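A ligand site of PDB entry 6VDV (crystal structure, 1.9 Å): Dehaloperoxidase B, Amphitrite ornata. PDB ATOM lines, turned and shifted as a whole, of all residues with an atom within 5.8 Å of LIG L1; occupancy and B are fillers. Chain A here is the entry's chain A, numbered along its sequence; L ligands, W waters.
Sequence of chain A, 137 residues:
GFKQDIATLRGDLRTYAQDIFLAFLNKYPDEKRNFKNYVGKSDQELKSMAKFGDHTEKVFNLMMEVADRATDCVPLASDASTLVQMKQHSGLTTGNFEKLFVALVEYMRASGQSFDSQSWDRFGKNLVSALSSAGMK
Phe 24 touches LIG L1 (CZ to C26, 3.7 Å). Glu 31 touches LIG L1. Asn 34 touches LIG L1 (O to C31, 3.5 Å). Phe 35 touches LIG L1 (CE1 to C31, 3.8 Å). CD of Lys 58 touches O2 of LIG L1, 3.5 Å away. Val 59 touches LIG L1 (O to C17, 3.2 Å). C of Leu 62 touches C17 of LIG L1, at 3.9 Å. N of Met 63 touches C17 of LIG L1 (3.3 Å). CE of Met 86 touches C8 of LIG L1, at 3.7 Å. Gln 88 touches LIG L1 (CB to C1, 3.7 Å). Leu 92 touches LIG L1. O of Asn 96 touches C24 of LIG L1, 3.3 Å away. CE2 of Phe 97 touches C3 of LIG L1 (3.2 Å). Leu 100 touches LIG L1. Phe 101 touches LIG L1. CD2 of Leu 127 touches C19 of LIG L1, at 3.5 Å.
The side-chain carboxylate (OD2) of Asp 54 lies within salt-bridge range of the side-chain amino group (NZ) of Lys 58 (3.1 Å). The side-chain carboxylate (OE2) of Glu 31 is in hydrogen-bond range of the side-chain amide nitrogen (ND2) of Asn 96 (2.8 Å). The backbone carbonyl oxygen (O) of Leu 83 sits at hydrogen-bond distance from a ring nitrogen (ND1) of His 89.
An oxygen (O4) of LIG L1 sits at hydrogen-bond distance from an oxygen (O1) of LG2 L2 (2.8 Å).
MN1 of LIG L1 is bound by NE2 of His 89. A ring nitrogen (ND1) of His 55 lies within hydrogen-bond range of an oxygen (O3) of LIG L1, 2.4 Å away. The side-chain hydroxyl (OH) of Tyr 38 sits at hydrogen-bond distance from an oxygen (O1) of LG2 L2 (3.1 Å).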
ATOM      1  N   PHE A  24      23.877  21.315   9.897  1.00  0.00           N
ATOM      2  CA  PHE A  24      23.856  20.097   9.103  1.00  0.00           C
ATOM      3  C   PHE A  24      22.883  20.238   7.936  1.00  0.00           C
ATOM      4  O   PHE A  24      23.255  20.010   6.776  1.00  0.00           O
ATOM      5  CB  PHE A  24      23.486  18.932  10.022  1.00  0.00           C
ATOM      6  CG  PHE A  24      23.034  17.695   9.320  1.00  0.00           C
ATOM      7  CD1 PHE A  24      23.922  16.940   8.568  1.00  0.00           C
ATOM      8  CD2 PHE A  24      21.725  17.250   9.452  1.00  0.00           C
ATOM      9  CE1 PHE A  24      23.510  15.759   7.945  1.00  0.00           C
ATOM     10  CE2 PHE A  24      21.290  16.080   8.831  1.00  0.00           C
ATOM     11  CZ  PHE A  24      22.188  15.325   8.081  1.00  0.00           C
ATOM     12  N   GLU A  31      19.785  16.236   2.571  1.00  0.00           N
ATOM     13  CA  GLU A  31      19.426  15.427   3.728  1.00  0.00           C
ATOM     14  C   GLU A  31      17.999  15.706   4.212  1.00  0.00           C
ATOM     15  O   GLU A  31      17.502  14.944   5.051  1.00  0.00           O
ATOM     16  CB  GLU A  31      20.429  15.650   4.856  1.00  0.00           C
ATOM     17  CG  GLU A  31      21.845  15.132   4.550  1.00  0.00           C
ATOM     18  CD  GLU A  31      21.967  13.617   4.689  1.00  0.00           C
ATOM     19  OE1 GLU A  31      22.457  12.958   3.755  1.00  0.00           O
ATOM     20  OE2 GLU A  31      21.549  13.078   5.738  1.00  0.00           O
ATOM     21  N   ASN A  34      14.954  13.056   4.488  1.00  0.00           N
ATOM     22  CA  ASN A  34      14.521  12.377   5.695  1.00  0.00           C
ATOM     23  C   ASN A  34      13.798  13.286   6.666  1.00  0.00           C
ATOM     24  O   ASN A  34      13.423  12.835   7.764  1.00  0.00           O
ATOM     25  CB  ASN A  34      15.712  11.718   6.397  1.00  0.00           C
ATOM     26  CG  ASN A  34      16.256  10.518   5.642  1.00  0.00           C
ATOM     27  OD1 ASN A  34      15.488   9.722   5.091  1.00  0.00           O
ATOM     28  ND2 ASN A  34      17.571  10.394   5.599  1.00  0.00           N
ATOM     29  N   PHE A  35      13.583  14.552   6.301  1.00  0.00           N
ATOM     30  CA  PHE A  35      12.937  15.536   7.172  1.00  0.00           C
ATOM     31  C   PHE A  35      11.943  16.372   6.357  1.00  0.00           C
ATOM     32  O   PHE A  35      12.037  17.603   6.273  1.00  0.00           O
ATOM     33  CB  PHE A  35      13.976  16.428   7.857  1.00  0.00           C
ATOM     34  CG  PHE A  35      15.018  15.661   8.620  1.00  0.00           C
ATOM     35  CD1 PHE A  35      14.709  15.071   9.842  1.00  0.00           C
ATOM     36  CD2 PHE A  35      16.310  15.545   8.129  1.00  0.00           C
ATOM     37  CE1 PHE A  35      15.675  14.370  10.554  1.00  0.00           C
ATOM     38  CE2 PHE A  35      17.285  14.835   8.847  1.00  0.00           C
ATOM     39  CZ  PHE A  35      16.966  14.264  10.060  1.00  0.00           C
ATOM     40  N   TYR A  38      10.488  19.693   7.474  1.00  0.00           N
ATOM     41  CA  TYR A  38      11.373  20.830   7.702  1.00  0.00           C
ATOM     42  C   TYR A  38      11.658  21.603   6.430  1.00  0.00           C
ATOM     43  O   TYR A  38      12.379  22.608   6.474  1.00  0.00           O
ATOM     44  CB  TYR A  38      12.681  20.368   8.362  1.00  0.00           C
ATOM     45  CG  TYR A  38      12.479  19.719   9.725  1.00  0.00           C
ATOM     46  CD1 TYR A  38      11.325  19.947  10.475  1.00  0.00           C
ATOM     47  CD2 TYR A  38      13.445  18.869  10.258  1.00  0.00           C
ATOM     48  CE1 TYR A  38      11.148  19.343  11.712  1.00  0.00           C
ATOM     49  CE2 TYR A  38      13.268  18.264  11.495  1.00  0.00           C
ATOM     50  CZ  TYR A  38      12.119  18.506  12.220  1.00  0.00           C
ATOM     51  OH  TYR A  38      11.956  17.887  13.444  1.00  0.00           O
ATOM     52  N   ASP A  54      11.735  19.962  20.043  1.00  0.00           N
ATOM     53  CA  ASP A  54      11.644  18.817  20.950  1.00  0.00           C
ATOM     54  C   ASP A  54      12.407  17.614  20.412  1.00  0.00           C
ATOM     55  O   ASP A  54      13.126  16.933  21.164  1.00  0.00           O
ATOM     56  CB  ASP A  54      10.180  18.466  21.187  1.00  0.00           C
ATOM     57  CG  ASP A  54      10.014  17.317  22.153  1.00  0.00           C
ATOM     58  OD1 ASP A  54      10.352  17.477  23.338  1.00  0.00           O
ATOM     59  OD2 ASP A  54       9.553  16.244  21.710  1.00  0.00           O
ATOM     60  N   HIS A  55      12.270  17.316  19.114  1.00  0.00           N
ATOM     61  CA  HIS A  55      12.964  16.155  18.546  1.00  0.00           C
ATOM     62  C   HIS A  55      14.471  16.384  18.486  1.00  0.00           C
ATOM     63  O   HIS A  55      15.243  15.454  18.769  1.00  0.00           O
ATOM     64  CB  HIS A  55      12.440  15.852  17.142  1.00  0.00           C
ATOM     65  CG  HIS A  55      11.099  15.175  17.133  1.00  0.00           C
ATOM     66  ND1 HIS A  55      10.809  14.134  16.282  1.00  0.00           N
ATOM     67  CD2 HIS A  55       9.984  15.404  17.849  1.00  0.00           C
ATOM     68  CE1 HIS A  55       9.563  13.741  16.479  1.00  0.00           C
ATOM     69  NE2 HIS A  55       9.041  14.499  17.429  1.00  0.00           N
ATOM     70  N   LYS A  58      15.937  15.978  21.899  1.00  0.00           N
ATOM     71  CA  LYS A  58      15.950  14.573  22.299  1.00  0.00           C
ATOM     72  C   LYS A  58      17.049  13.797  21.574  1.00  0.00           C
ATOM     73  O   LYS A  58      17.697  12.919  22.165  1.00  0.00           O
ATOM     74  CB  LYS A  58      14.566  13.956  22.046  1.00  0.00           C
ATOM     75  CG  LYS A  58      13.562  14.341  23.129  1.00  0.00           C
ATOM     76  CD  LYS A  58      12.197  13.764  22.869  1.00  0.00           C
ATOM     77  CE  LYS A  58      11.272  14.024  24.053  1.00  0.00           C
ATOM     78  NZ  LYS A  58       9.837  13.833  23.689  1.00  0.00           N
ATOM     79  N   VAL A  59      17.263  14.094  20.290  1.00  0.00           N
ATOM     80  CA  VAL A  59      18.373  13.491  19.547  1.00  0.00           C
ATOM     81  C   VAL A  59      19.692  13.785  20.248  1.00  0.00           C
ATOM     82  O   VAL A  59      20.540  12.911  20.404  1.00  0.00           O
ATOM     83  CB  VAL A  59      18.388  14.018  18.100  1.00  0.00           C
ATOM     84  CG1 VAL A  59      19.718  13.670  17.430  1.00  0.00           C
ATOM     85  CG2 VAL A  59      17.217  13.452  17.293  1.00  0.00           C
ATOM     86  N   PHE A  60      19.876  15.038  20.674  1.00  0.00           N
ATOM     87  CA  PHE A  60      21.152  15.413  21.265  1.00  0.00           C
ATOM     88  C   PHE A  60      21.260  14.994  22.720  1.00  0.00           C
ATOM     89  O   PHE A  60      22.377  14.745  23.193  1.00  0.00           O
ATOM     90  CB  PHE A  60      21.389  16.921  21.089  1.00  0.00           C
ATOM     91  CG  PHE A  60      21.977  17.262  19.766  1.00  0.00           C
ATOM     92  CD1 PHE A  60      21.215  17.190  18.609  1.00  0.00           C
ATOM     93  CD2 PHE A  60      23.319  17.612  19.661  1.00  0.00           C
ATOM     94  CE1 PHE A  60      21.768  17.493  17.365  1.00  0.00           C
ATOM     95  CE2 PHE A  60      23.873  17.905  18.419  1.00  0.00           C
ATOM     96  CZ  PHE A  60      23.096  17.847  17.276  1.00  0.00           C
ATOM     97  N   LEU A  62      20.368  12.086  23.709  1.00  0.00           N
ATOM     98  CA  LEU A  62      20.910  10.734  23.612  1.00  0.00           C
ATOM     99  C   LEU A  62      22.324  10.740  23.038  1.00  0.00           C
ATOM    100  O   LEU A  62      23.170   9.936  23.452  1.00  0.00           O
ATOM    101  CB  LEU A  62      19.993   9.851  22.751  1.00  0.00           C
ATOM    102  CG  LEU A  62      20.403   8.390  22.547  1.00  0.00           C
ATOM    103  CD1 LEU A  62      20.582   7.655  23.891  1.00  0.00           C
ATOM    104  CD2 LEU A  62      19.380   7.670  21.641  1.00  0.00           C
ATOM    105  N   MET A  63      22.602  11.629  22.073  1.00  0.00           N
ATOM    106  CA  MET A  63      23.973  11.710  21.573  1.00  0.00           C
ATOM    107  C   MET A  63      24.959  11.989  22.712  1.00  0.00           C
ATOM    108  O   MET A  63      26.046  11.397  22.755  1.00  0.00           O
ATOM    109  CB  MET A  63      24.091  12.777  20.481  1.00  0.00           C
ATOM    110  CG  MET A  63      25.447  12.739  19.766  1.00  0.00           C
ATOM    111  SD  MET A  63      25.910  14.300  18.975  1.00  0.00           S
ATOM    112  CE  MET A  63      24.703  14.368  17.643  1.00  0.00           C
ATOM    113  N   VAL A  66      25.465   8.822  24.709  1.00  0.00           N
ATOM    114  CA  VAL A  66      26.353   7.888  24.022  1.00  0.00           C
ATOM    115  C   VAL A  66      27.796   8.369  24.106  1.00  0.00           C
ATOM    116  O   VAL A  66      28.724   7.569  24.292  1.00  0.00           O
ATOM    117  CB  VAL A  66      25.905   7.684  22.565  1.00  0.00           C
ATOM    118  CG1 VAL A  66      26.934   6.817  21.818  1.00  0.00           C
ATOM    119  CG2 VAL A  66      24.509   7.053  22.506  1.00  0.00           C
ATOM    120  N   LEU A  83      21.016   2.435  18.112  1.00  0.00           N
ATOM    121  CA  LEU A  83      20.878   3.392  17.012  1.00  0.00           C
ATOM    122  C   LEU A  83      20.564   2.696  15.684  1.00  0.00           C
ATOM    123  O   LEU A  83      19.852   3.258  14.851  1.00  0.00           O
ATOM    124  CB  LEU A  83      22.156   4.215  16.885  1.00  0.00           C
ATOM    125  CG  LEU A  83      22.442   5.139  18.072  1.00  0.00           C
ATOM    126  CD1 LEU A  83      23.855   5.732  17.974  1.00  0.00           C
ATOM    127  CD2 LEU A  83      21.399   6.250  18.149  1.00  0.00           C
ATOM    128  N   MET A  86      16.636   1.236  16.118  1.00  0.00           N
ATOM    129  CA  MET A  86      15.527   2.179  16.231  1.00  0.00           C
ATOM    130  C   MET A  86      14.726   2.201  14.939  1.00  0.00           C
ATOM    131  O   MET A  86      15.293   2.280  13.852  1.00  0.00           O
ATOM    132  CB  MET A  86      16.055   3.578  16.537  1.00  0.00           C
ATOM    133  CG  MET A  86      16.558   3.774  17.936  1.00  0.00           C
ATOM    134  SD  MET A  86      17.424   5.365  18.041  1.00  0.00           S
ATOM    135  CE  MET A  86      16.158   6.499  17.455  1.00  0.00           C
ATOM    136  N   GLN A  88      12.878   4.599  13.928  1.00  0.00           N
ATOM    137  CA  GLN A  88      13.043   5.932  13.358  1.00  0.00           C
ATOM    138  C   GLN A  88      14.235   6.011  12.416  1.00  0.00           C
ATOM    139  O   GLN A  88      14.312   6.934  11.605  1.00  0.00           O
ATOM    140  CB  GLN A  88      13.201   6.951  14.483  1.00  0.00           C
ATOM    141  CG  GLN A  88      12.105   6.888  15.541  1.00  0.00           C
ATOM    142  CD  GLN A  88      12.419   5.936  16.684  1.00  0.00           C
ATOM    143  OE1 GLN A  88      12.933   4.843  16.480  1.00  0.00           O
ATOM    144  NE2 GLN A  88      12.110   6.362  17.906  1.00  0.00           N
ATOM    145  N   HIS A  89      15.179   5.074  12.530  1.00  0.00           N
ATOM    146  CA  HIS A  89      16.376   5.031  11.702  1.00  0.00           C
ATOM    147  C   HIS A  89      16.308   3.997  10.592  1.00  0.00           C
ATOM    148  O   HIS A  89      17.335   3.693   9.974  1.00  0.00           O
ATOM    149  CB  HIS A  89      17.605   4.744  12.558  1.00  0.00           C
ATOM    150  CG  HIS A  89      17.964   5.852  13.491  1.00  0.00           C
ATOM    151  ND1 HIS A  89      18.963   5.747  14.439  1.00  0.00           N
ATOM    152  CD2 HIS A  89      17.455   7.099  13.617  1.00  0.00           C
ATOM    153  CE1 HIS A  89      19.049   6.878  15.114  1.00  0.00           C
ATOM    154  NE2 HIS A  89      18.141   7.716  14.643  1.00  0.00           N
ATOM    155  N   LEU A  92      18.119   4.742   7.204  1.00  0.00           N
ATOM    156  CA  LEU A  92      19.355   5.516   7.190  1.00  0.00           C
ATOM    157  C   LEU A  92      20.578   4.629   6.917  1.00  0.00           C
ATOM    158  O   LEU A  92      20.575   3.419   7.135  1.00  0.00           O
ATOM    159  CB  LEU A  92      19.543   6.251   8.517  1.00  0.00           C
ATOM    160  CG  LEU A  92      18.378   7.066   9.063  1.00  0.00           C
ATOM    161  CD1 LEU A  92      18.770   7.650  10.402  1.00  0.00           C
ATOM    162  CD2 LEU A  92      17.997   8.150   8.079  1.00  0.00           C
ATOM    163  N   ASN A  96      24.677   9.198   6.478  1.00  0.00           N
ATOM    164  CA  ASN A  96      23.842  10.206   7.133  1.00  0.00           C
ATOM    165  C   ASN A  96      24.480  10.685   8.425  1.00  0.00           C
ATOM    166  O   ASN A  96      24.444  11.874   8.752  1.00  0.00           O
ATOM    167  CB  ASN A  96      22.443   9.643   7.430  1.00  0.00           C
ATOM    168  CG  ASN A  96      21.652   9.310   6.174  1.00  0.00           C
ATOM    169  OD1 ASN A  96      21.279   8.152   5.962  1.00  0.00           O
ATOM    170  ND2 ASN A  96      21.338  10.327   5.376  1.00  0.00           N
ATOM    171  N   PHE A  97      25.074   9.753   9.181  1.00  0.00           N
ATOM    172  CA  PHE A  97      25.686  10.110  10.450  1.00  0.00           C
ATOM    173  C   PHE A  97      27.031  10.797  10.253  1.00  0.00           C
ATOM    174  O   PHE A  97      27.382  11.688  11.025  1.00  0.00           O
ATOM    175  CB  PHE A  97      25.852   8.848  11.307  1.00  0.00           C
ATOM    176  CG  PHE A  97      24.565   8.294  11.832  1.00  0.00           C
ATOM    177  CD1 PHE A  97      23.676   7.638  10.994  1.00  0.00           C
ATOM    178  CD2 PHE A  97      24.241   8.434  13.181  1.00  0.00           C
ATOM    179  CE1 PHE A  97      22.495   7.119  11.493  1.00  0.00           C
ATOM    180  CE2 PHE A  97      23.060   7.915  13.680  1.00  0.00           C
ATOM    181  CZ  PHE A  97      22.183   7.257  12.834  1.00  0.00           C
ATOM    182  N   LEU A 100      26.307  14.437   9.562  1.00  0.00           N
ATOM    183  CA  LEU A 100      25.991  15.113  10.814  1.00  0.00           C
ATOM    184  C   LEU A 100      27.258  15.471  11.590  1.00  0.00           C
ATOM    185  O   LEU A 100      27.412  16.601  12.057  1.00  0.00           O
ATOM    186  CB  LEU A 100      25.051  14.250  11.649  1.00  0.00           C
ATOM    187  CG  LEU A 100      24.609  14.828  12.997  1.00  0.00           C
ATOM    188  CD1 LEU A 100      23.852  16.135  12.785  1.00  0.00           C
ATOM    189  CD2 LEU A 100      23.751  13.825  13.745  1.00  0.00           C
ATOM    190  N   PHE A 101      28.208  14.528  11.685  1.00  0.00           N
ATOM    191  CA  PHE A 101      29.388  14.824  12.501  1.00  0.00           C
ATOM    192  C   PHE A 101      30.403  15.694  11.790  1.00  0.00           C
ATOM    193  O   PHE A 101      31.206  16.342  12.469  1.00  0.00           O
ATOM    194  CB  PHE A 101      30.026  13.525  13.014  1.00  0.00           C
ATOM    195  CG  PHE A 101      29.289  12.991  14.198  1.00  0.00           C
ATOM    196  CD1 PHE A 101      29.584  13.448  15.464  1.00  0.00           C
ATOM    197  CD2 PHE A 101      28.223  12.133  14.033  1.00  0.00           C
ATOM    198  CE1 PHE A 101      28.860  13.013  16.556  1.00  0.00           C
ATOM    199  CE2 PHE A 101      27.501  11.695  15.116  1.00  0.00           C
ATOM    200  CZ  PHE A 101      27.821  12.138  16.371  1.00  0.00           C
ATOM    201  N   PHE A 123      35.126  10.688  17.507  1.00  0.00           N
ATOM    202  CA  PHE A 123      33.868  10.103  17.963  1.00  0.00           C
ATOM    203  C   PHE A 123      32.942   9.804  16.792  1.00  0.00           C
ATOM    204  O   PHE A 123      32.364   8.710  16.692  1.00  0.00           O
ATOM    205  CB  PHE A 123      33.188  11.050  18.955  1.00  0.00           C
ATOM    206  CG  PHE A 123      31.852  10.559  19.450  1.00  0.00           C
ATOM    207  CD1 PHE A 123      31.759   9.342  20.121  1.00  0.00           C
ATOM    208  CD2 PHE A 123      30.711  11.285  19.234  1.00  0.00           C
ATOM    209  CE1 PHE A 123      30.534   8.870  20.572  1.00  0.00           C
ATOM    210  CE2 PHE A 123      29.467  10.812  19.680  1.00  0.00           C
ATOM    211  CZ  PHE A 123      29.383   9.605  20.351  1.00  0.00           C
ATOM    212  N   LEU A 127      31.843   6.223  15.741  1.00  0.00           N
ATOM    213  CA  LEU A 127      30.426   5.888  15.759  1.00  0.00           C
ATOM    214  C   LEU A 127      30.015   5.245  14.434  1.00  0.00           C
ATOM    215  O   LEU A 127      29.329   4.210  14.429  1.00  0.00           O
ATOM    216  CB  LEU A 127      29.594   7.138  16.041  1.00  0.00           C
ATOM    217  CG  LEU A 127      28.075   6.899  16.068  1.00  0.00           C
ATOM    218  CD1 LEU A 127      27.661   5.924  17.166  1.00  0.00           C
ATOM    219  CD2 LEU A 127      27.333   8.221  16.243  1.00  0.00           C
HETATM  220  C1  LIG L   1      14.731  10.157  15.627  1.00  0.00           C
HETATM  221  C2  LIG L   1      18.684   9.882  18.083  1.00  0.00           C
HETATM  222  C3  LIG L   1      21.383  10.602  14.139  1.00  0.00           C
HETATM  223  C4  LIG L   1      17.181  10.644  11.413  1.00  0.00           C
HETATM  224  C5  LIG L   1      15.525  10.111  16.871  1.00  0.00           C
HETATM  225  C6  LIG L   1      15.161  10.094  18.086  1.00  0.00           C
HETATM  226  C7  LIG L   1      16.461   9.999  18.783  1.00  0.00           C
HETATM  227  C8  LIG L   1      17.352   9.985  17.752  1.00  0.00           C
HETATM  228  C9  LIG L   1      16.426   9.965  20.235  1.00  0.00           C
HETATM  229  C10 LIG L   1      13.632  10.192  18.631  1.00  0.00           C
HETATM  230  C11 LIG L   1      13.168  11.792  18.747  1.00  0.00           C
HETATM  231  C12 LIG L   1      11.753  11.857  19.213  1.00  0.00           C
HETATM  232  O1  LIG L   1      10.885  11.066  18.647  1.00  0.00           O
HETATM  233  O2  LIG L   1      11.508  12.847  19.580  1.00  0.00           O
HETATM  234  C13 LIG L   1      19.882  10.075  17.441  1.00  0.00           C
HETATM  235  C14 LIG L   1      21.174  10.212  17.635  1.00  0.00           C
HETATM  236  C15 LIG L   1      22.091  10.436  16.495  1.00  0.00           C
HETATM  237  C16 LIG L   1      21.182  10.422  15.466  1.00  0.00           C
HETATM  238  C17 LIG L   1      21.740  10.134  19.262  1.00  0.00           C
HETATM  239  C18 LIG L   1      23.261  10.585  16.494  1.00  0.00           C
HETATM  240  C19 LIG L   1      24.472  10.058  17.150  1.00  0.00           C
HETATM  241  C20 LIG L   1      20.477  10.745  13.042  1.00  0.00           C
HETATM  242  C21 LIG L   1      21.021  11.096  11.684  1.00  0.00           C
HETATM  243  C22 LIG L   1      19.652  11.091  10.871  1.00  0.00           C
HETATM  244  C23 LIG L   1      18.574  10.755  11.855  1.00  0.00           C
HETATM  245  C24 LIG L   1      22.306  11.350  11.271  1.00  0.00           C
HETATM  246  C25 LIG L   1      19.539  11.368   9.533  1.00  0.00           C
HETATM  247  C26 LIG L   1      20.253  12.295   8.814  1.00  0.00           C
HETATM  248  C27 LIG L   1      16.163  10.536  12.321  1.00  0.00           C
HETATM  249  C28 LIG L   1      14.846  10.608  12.164  1.00  0.00           C
HETATM  250  C29 LIG L   1      14.128  10.526  13.009  1.00  0.00           C
HETATM  251  C30 LIG L   1      14.970  10.304  14.330  1.00  0.00           C
HETATM  252  C31 LIG L   1      14.346  10.854  10.502  1.00  0.00           C
HETATM  253  C32 LIG L   1      12.498  10.523  13.400  1.00  0.00           C
HETATM  254  C33 LIG L   1      11.821  11.566  12.837  1.00  0.00           C
HETATM  255  C34 LIG L   1      12.209  13.003  13.613  1.00  0.00           C
HETATM  256  O3  LIG L   1      12.300  12.974  14.773  1.00  0.00           O
HETATM  257  O4  LIG L   1      12.239  13.907  12.742  1.00  0.00           O
HETATM  258 MN1  LIG L   1      17.970  10.040  14.890  1.00  0.00          MN
HETATM  259  N1  LIG L   1      16.834  10.063  16.599  1.00  0.00           N
HETATM  260  N2  LIG L   1      19.693  10.223  15.758  1.00  0.00           N
HETATM  261  N3  LIG L   1      19.003  10.520  13.184  1.00  0.00           N
HETATM  262  N4  LIG L   1      16.272  10.357  13.639  1.00  0.00           N
HETATM  263  O1  LG2 L   2      13.874  15.579  14.337  1.00  0.00           O
HETATM  264  C1  LG2 L   2      15.257  15.307  14.184  1.00  0.00           C
HETATM  265  C2  LG2 L   2      15.716  14.029  13.926  1.00  0.00           C
HETATM  266  C3  LG2 L   2      17.086  13.788  13.771  1.00  0.00           C
HETATM  267  C4  LG2 L   2      17.985  14.836  13.879  1.00  0.00           C
HETATM  268  C5  LG2 L   2      17.513  16.107  14.148  1.00  0.00           C
HETATM  269  C6  LG2 L   2      16.155  16.346  14.295  1.00  0.00           C
HETATM  270 BR1  LG2 L   2      19.905  14.563  13.668  1.00  0.00          BR
HETATM  271  O   HOH W   1       8.557  10.178  18.435  1.00  0.00           O
